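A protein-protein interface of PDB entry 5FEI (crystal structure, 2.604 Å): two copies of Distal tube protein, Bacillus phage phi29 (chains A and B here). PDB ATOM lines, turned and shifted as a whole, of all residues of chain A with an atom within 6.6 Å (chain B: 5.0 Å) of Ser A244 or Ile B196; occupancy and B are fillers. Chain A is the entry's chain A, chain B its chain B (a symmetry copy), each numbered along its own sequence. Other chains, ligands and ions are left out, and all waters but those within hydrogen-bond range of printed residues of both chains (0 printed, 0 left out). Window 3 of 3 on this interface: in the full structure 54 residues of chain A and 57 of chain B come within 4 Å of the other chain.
N of Ala B198 is in hydrogen-bond range of OG1 of Thr A240, 3.1 Å away.
The backbone carbonyl oxygen of Thr A240 is in hydrogen-bond range of the side-chain hydroxyl of Ser A244.
Among the printed residues, pairs that only touch across the chains: Leu A409 with Ile B196, Thr A240 with Ile B196, Leu A239 with Ala B198, Ser A244 with Ile B196, Leu A409 with Lys B179 and Phe A243 with Ile B196.
Printed residues of chain B within 4 Å of Leu A239: Ala B198 (3.6 Å).
Of chain B, only Ile B196 (3.7 Å) comes within 4 Å of Ser A244.
Gln A245 touches none of the printed residues of chain B.
Ile B196 touches four residues of chain A.
Printed residues of chain A within 4 Å of Ala B198: Leu A239 (3.6 Å) and Thr A240 (3.1 Å).
The nearest printed residue of chain B that does not touch Ser A244 is Asp B195 (5.9 Å).
The nearest printed residue of chain B that does not touch Leu A409 is Pro B206 (4.1 Å).
Of the 14 printed residues of chain A, 5 touch a printed residue of chain B.
Printed residues of chain B that touch a printed residue of chain A: Lys B179, Ile B196 and Ala B198.
Hydrophobic or aromatic side chains of chain B within 4 Å of the printed part of chain A: Ile B196 and Ala B198.
Among the printed residues, 7 pairs touch across the chains.
Among the printed residues, no Asp or Glu carboxylate lies within 4 Å of a Lys or Arg side-chain nitrogen of the other chain.
No position is printed for both chains.
Of the 7 pairs that touch across the chains among the printed residues, none has its exchanged pair printed and touching as well.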
ATOM      1  N   LEU A 239       5.687  16.955   7.638  1.00  0.00           N
ATOM      2  CA  LEU A 239       6.845  16.602   8.462  1.00  0.00           C
ATOM      3  C   LEU A 239       7.715  17.813   8.785  1.00  0.00           C
ATOM      4  O   LEU A 239       8.120  18.012   9.935  1.00  0.00           O
ATOM      5  CB  LEU A 239       7.699  15.533   7.786  1.00  0.00           C
ATOM      6  CG  LEU A 239       7.110  14.124   7.731  1.00  0.00           C
ATOM      7  CD1 LEU A 239       8.153  13.129   7.198  1.00  0.00           C
ATOM      8  CD2 LEU A 239       6.591  13.703   9.090  1.00  0.00           C
ATOM      9  N   THR A 240       8.038  18.605   7.771  1.00  0.00           N
ATOM     10  CA  THR A 240       8.858  19.777   8.011  1.00  0.00           C
ATOM     11  C   THR A 240       8.232  20.683   9.074  1.00  0.00           C
ATOM     12  O   THR A 240       8.901  21.154   9.992  1.00  0.00           O
ATOM     13  CB  THR A 240       9.052  20.584   6.725  1.00  0.00           C
ATOM     14  OG1 THR A 240       9.791  19.800   5.780  1.00  0.00           O
ATOM     15  CG2 THR A 240       9.788  21.903   7.013  1.00  0.00           C
ATOM     16  N   ASN A 241       6.932  20.899   8.962  1.00  0.00           N
ATOM     17  CA  ASN A 241       6.279  21.879   9.809  1.00  0.00           C
ATOM     18  C   ASN A 241       6.072  21.318  11.199  1.00  0.00           C
ATOM     19  O   ASN A 241       6.267  22.010  12.198  1.00  0.00           O
ATOM     20  CB  ASN A 241       4.970  22.347   9.167  1.00  0.00           C
ATOM     21  CG  ASN A 241       5.223  23.247   7.949  1.00  0.00           C
ATOM     22  OD1 ASN A 241       6.208  23.993   7.909  1.00  0.00           O
ATOM     23  ND2 ASN A 241       4.352  23.162   6.952  1.00  0.00           N
ATOM     24  N   ILE A 242       5.690  20.053  11.260  1.00  0.00           N
ATOM     25  CA  ILE A 242       5.452  19.413  12.539  1.00  0.00           C
ATOM     26  C   ILE A 242       6.714  19.446  13.405  1.00  0.00           C
ATOM     27  O   ILE A 242       6.624  19.655  14.613  1.00  0.00           O
ATOM     28  CB  ILE A 242       4.974  17.963  12.363  1.00  0.00           C
ATOM     29  CG1 ILE A 242       4.251  17.498  13.614  1.00  0.00           C
ATOM     30  CG2 ILE A 242       6.141  17.044  12.056  1.00  0.00           C
ATOM     31  CD1 ILE A 242       3.013  18.286  13.887  1.00  0.00           C
ATOM     32  N   PHE A 243       7.889  19.253  12.803  1.00  0.00           N
ATOM     33  CA  PHE A 243       9.122  19.202  13.598  1.00  0.00           C
ATOM     34  C   PHE A 243       9.743  20.565  13.801  1.00  0.00           C
ATOM     35  O   PHE A 243      10.739  20.697  14.495  1.00  0.00           O
ATOM     36  CB  PHE A 243      10.133  18.233  12.968  1.00  0.00           C
ATOM     37  CG  PHE A 243       9.792  16.786  13.209  1.00  0.00           C
ATOM     38  CD1 PHE A 243       9.938  16.235  14.476  1.00  0.00           C
ATOM     39  CD2 PHE A 243       9.266  15.998  12.200  1.00  0.00           C
ATOM     40  CE1 PHE A 243       9.592  14.903  14.729  1.00  0.00           C
ATOM     41  CE2 PHE A 243       8.914  14.665  12.443  1.00  0.00           C
ATOM     42  CZ  PHE A 243       9.079  14.119  13.712  1.00  0.00           C
ATOM     43  N   SER A 244       9.119  21.583  13.224  1.00  0.00           N
ATOM     44  CA  SER A 244       9.593  22.955  13.344  1.00  0.00           C
ATOM     45  C   SER A 244       8.979  23.653  14.550  1.00  0.00           C
ATOM     46  O   SER A 244       9.441  24.710  14.971  1.00  0.00           O
ATOM     47  CB  SER A 244       9.270  23.741  12.077  1.00  0.00           C
ATOM     48  OG  SER A 244      10.186  23.446  11.043  1.00  0.00           O
ATOM     49  N   GLN A 245       7.940  23.052  15.111  1.00  0.00           N
ATOM     50  CA  GLN A 245       7.227  23.656  16.226  1.00  0.00           C
ATOM     51  C   GLN A 245       7.808  23.069  17.492  1.00  0.00           C
ATOM     52  O   GLN A 245       7.700  21.873  17.738  1.00  0.00           O
ATOM     53  CB  GLN A 245       5.724  23.392  16.123  1.00  0.00           C
ATOM     54  CG  GLN A 245       5.111  23.843  14.796  1.00  0.00           C
ATOM     55  CD  GLN A 245       3.590  23.812  14.808  1.00  0.00           C
ATOM     56  OE1 GLN A 245       2.973  23.557  15.846  1.00  0.00           O
ATOM     57  NE2 GLN A 245       2.977  24.077  13.655  1.00  0.00           N
ATOM     58  N   LYS A 246       8.422  23.922  18.298  1.00  0.00           N
ATOM     59  CA  LYS A 246       9.153  23.458  19.467  1.00  0.00           C
ATOM     60  C   LYS A 246       8.248  22.832  20.523  1.00  0.00           C
ATOM     61  O   LYS A 246       8.707  22.042  21.347  1.00  0.00           O
ATOM     62  CB  LYS A 246       9.955  24.613  20.081  1.00  0.00           C
ATOM     63  CG  LYS A 246      11.009  24.151  21.086  1.00  0.00           C
ATOM     64  CD  LYS A 246      12.004  23.197  20.401  1.00  0.00           C
ATOM     65  CE  LYS A 246      12.803  22.363  21.397  1.00  0.00           C
ATOM     66  NZ  LYS A 246      13.737  23.185  22.210  1.00  0.00           N
ATOM     67  N   SER A 247       6.955  23.124  20.463  1.00  0.00           N
ATOM     68  CA  SER A 247       6.043  22.606  21.473  1.00  0.00           C
ATOM     69  C   SER A 247       5.586  21.214  21.071  1.00  0.00           C
ATOM     70  O   SER A 247       5.405  20.334  21.915  1.00  0.00           O
ATOM     71  CB  SER A 247       4.836  23.537  21.651  1.00  0.00           C
ATOM     72  OG  SER A 247       4.137  23.711  20.430  1.00  0.00           O
ATOM     73  N   VAL A 249       7.365  19.046  19.175  1.00  0.00           N
ATOM     74  CA  VAL A 249       8.427  18.036  19.177  1.00  0.00           C
ATOM     75  C   VAL A 249       8.747  17.515  20.564  1.00  0.00           C
ATOM     76  O   VAL A 249       9.347  16.445  20.698  1.00  0.00           O
ATOM     77  CB  VAL A 249       9.749  18.568  18.570  1.00  0.00           C
ATOM     78  CG1 VAL A 249       9.581  18.852  17.089  1.00  0.00           C
ATOM     79  CG2 VAL A 249      10.236  19.806  19.322  1.00  0.00           C
ATOM     80  N   ASP A 288       1.449  26.996  14.506  1.00  0.00           N
ATOM     81  CA  ASP A 288       2.567  27.604  15.214  1.00  0.00           C
ATOM     82  C   ASP A 288       2.428  29.128  15.201  1.00  0.00           C
ATOM     83  O   ASP A 288       2.773  29.806  16.172  1.00  0.00           O
ATOM     84  CB  ASP A 288       3.892  27.170  14.577  1.00  0.00           C
ATOM     85  CG  ASP A 288       5.066  27.296  15.525  1.00  0.00           C
ATOM     86  OD1 ASP A 288       4.856  27.148  16.749  1.00  0.00           O
ATOM     87  OD2 ASP A 288       6.199  27.521  15.045  1.00  0.00           O
ATOM     88  N   HIS A 291       5.619  29.093  11.977  1.00  0.00           N
ATOM     89  CA  HIS A 291       5.870  28.157  10.882  1.00  0.00           C
ATOM     90  C   HIS A 291       4.532  27.728  10.278  1.00  0.00           C
ATOM     91  O   HIS A 291       3.484  27.895  10.913  1.00  0.00           O
ATOM     92  CB  HIS A 291       6.691  26.964  11.381  1.00  0.00           C
ATOM     93  CG  HIS A 291       8.059  27.346  11.858  1.00  0.00           C
ATOM     94  ND1 HIS A 291       8.338  27.622  13.183  1.00  0.00           N
ATOM     95  CD2 HIS A 291       9.216  27.557  11.186  1.00  0.00           C
ATOM     96  CE1 HIS A 291       9.608  27.955  13.306  1.00  0.00           C
ATOM     97  NE2 HIS A 291      10.167  27.925  12.106  1.00  0.00           N
ATOM     98  N   GLY A 292       4.557  27.194   9.057  1.00  0.00           N
ATOM     99  CA  GLY A 292       3.312  26.892   8.371  1.00  0.00           C
ATOM    100  C   GLY A 292       2.416  25.884   9.072  1.00  0.00           C
ATOM    101  O   GLY A 292       2.876  25.049   9.860  1.00  0.00           O
ATOM    102  N   LEU A 409      13.067  14.297  15.978  1.00  0.00           N
ATOM    103  CA  LEU A 409      13.965  15.403  16.325  1.00  0.00           C
ATOM    104  C   LEU A 409      13.756  15.925  17.756  1.00  0.00           C
ATOM    105  O   LEU A 409      14.535  15.609  18.671  1.00  0.00           O
ATOM    106  CB  LEU A 409      13.812  16.534  15.307  1.00  0.00           C
ATOM    107  CG  LEU A 409      14.466  16.264  13.936  1.00  0.00           C
ATOM    108  CD1 LEU A 409      14.264  14.852  13.420  1.00  0.00           C
ATOM    109  CD2 LEU A 409      14.040  17.284  12.883  1.00  0.00           C
ATOM    110  N   LYS B 179      20.245  16.751  11.714  1.00  0.00           N
ATOM    111  CA  LYS B 179      18.901  17.066  12.144  1.00  0.00           C
ATOM    112  C   LYS B 179      18.369  18.276  11.388  1.00  0.00           C
ATOM    113  O   LYS B 179      17.159  18.435  11.222  1.00  0.00           O
ATOM    114  CB  LYS B 179      18.878  17.296  13.658  1.00  0.00           C
ATOM    115  CG  LYS B 179      19.062  15.997  14.450  1.00  0.00           C
ATOM    116  CD  LYS B 179      18.748  16.120  15.947  1.00  0.00           C
ATOM    117  CE  LYS B 179      19.968  16.527  16.762  1.00  0.00           C
ATOM    118  NZ  LYS B 179      19.910  16.032  18.174  1.00  0.00           N
ATOM    119  N   SER B 180      19.269  19.124  10.910  1.00  0.00           N
ATOM    120  CA  SER B 180      18.827  20.327  10.214  1.00  0.00           C
ATOM    121  C   SER B 180      19.821  20.837   9.171  1.00  0.00           C
ATOM    122  O   SER B 180      20.943  20.329   9.047  1.00  0.00           O
ATOM    123  CB  SER B 180      18.534  21.427  11.232  1.00  0.00           C
ATOM    124  OG  SER B 180      19.730  21.820  11.877  1.00  0.00           O
ATOM    125  N   ASN B 194      19.983  25.802  10.091  1.00  0.00           N
ATOM    126  CA  ASN B 194      19.229  25.242  11.217  1.00  0.00           C
ATOM    127  C   ASN B 194      17.731  25.056  10.946  1.00  0.00           C
ATOM    128  O   ASN B 194      16.961  24.754  11.861  1.00  0.00           O
ATOM    129  CB  ASN B 194      19.427  26.090  12.473  1.00  0.00           C
ATOM    130  CG  ASN B 194      20.846  26.001  13.007  1.00  0.00           C
ATOM    131  OD1 ASN B 194      21.267  24.946  13.489  1.00  0.00           O
ATOM    132  ND2 ASN B 194      21.590  27.106  12.929  1.00  0.00           N
ATOM    133  N   ASP B 195      17.314  25.215   9.694  1.00  0.00           N
ATOM    134  CA  ASP B 195      15.940  24.886   9.345  1.00  0.00           C
ATOM    135  C   ASP B 195      15.796  23.372   9.267  1.00  0.00           C
ATOM    136  O   ASP B 195      16.712  22.663   8.818  1.00  0.00           O
ATOM    137  CB  ASP B 195      15.516  25.516   8.018  1.00  0.00           C
ATOM    138  CG  ASP B 195      15.306  27.022   8.107  1.00  0.00           C
ATOM    139  OD1 ASP B 195      15.447  27.619   9.209  1.00  0.00           O
ATOM    140  OD2 ASP B 195      14.956  27.601   7.056  1.00  0.00           O
ATOM    141  N   ILE B 196      14.657  22.883   9.738  1.00  0.00           N
ATOM    142  CA  ILE B 196      14.248  21.498   9.533  1.00  0.00           C
ATOM    143  C   ILE B 196      13.911  21.311   8.058  1.00  0.00           C
ATOM    144  O   ILE B 196      13.268  22.169   7.451  1.00  0.00           O
ATOM    145  CB  ILE B 196      13.016  21.142  10.414  1.00  0.00           C
ATOM    146  CG1 ILE B 196      13.366  21.301  11.888  1.00  0.00           C
ATOM    147  CG2 ILE B 196      12.517  19.731  10.142  1.00  0.00           C
ATOM    148  CD1 ILE B 196      14.620  20.571  12.268  1.00  0.00           C
ATOM    149  N   ASN B 197      14.343  20.209   7.470  1.00  0.00           N
ATOM    150  CA  ASN B 197      14.007  19.946   6.078  1.00  0.00           C
ATOM    151  C   ASN B 197      13.700  18.470   5.879  1.00  0.00           C
ATOM    152  O   ASN B 197      14.591  17.622   5.896  1.00  0.00           O
ATOM    153  CB  ASN B 197      15.137  20.391   5.139  1.00  0.00           C
ATOM    154  CG  ASN B 197      14.713  20.397   3.667  1.00  0.00           C
ATOM    155  OD1 ASN B 197      14.954  19.437   2.935  1.00  0.00           O
ATOM    156  ND2 ASN B 197      14.104  21.489   3.231  1.00  0.00           N
ATOM    157  N   ALA B 198      12.421  18.163   5.750  1.00  0.00           N
ATOM    158  CA  ALA B 198      11.986  16.810   5.439  1.00  0.00           C
ATOM    159  C   ALA B 198      12.029  16.594   3.933  1.00  0.00           C
ATOM    160  O   ALA B 198      11.948  17.548   3.151  1.00  0.00           O
ATOM    161  CB  ALA B 198      10.588  16.562   5.976  1.00  0.00           C
ATOM    162  N   PRO B 206      12.422  13.040   7.946  1.00  0.00           N
ATOM    163  CA  PRO B 206      12.689  14.407   8.396  1.00  0.00           C
ATOM    164  C   PRO B 206      14.180  14.822   8.491  1.00  0.00           C
ATOM    165  O   PRO B 206      14.462  15.960   8.856  1.00  0.00           O
ATOM    166  CB  PRO B 206      12.034  14.415   9.770  1.00  0.00           C
ATOM    167  CG  PRO B 206      12.313  13.043  10.284  1.00  0.00           C
ATOM    168  CD  PRO B 206      12.349  12.110   9.086  1.00  0.00           C
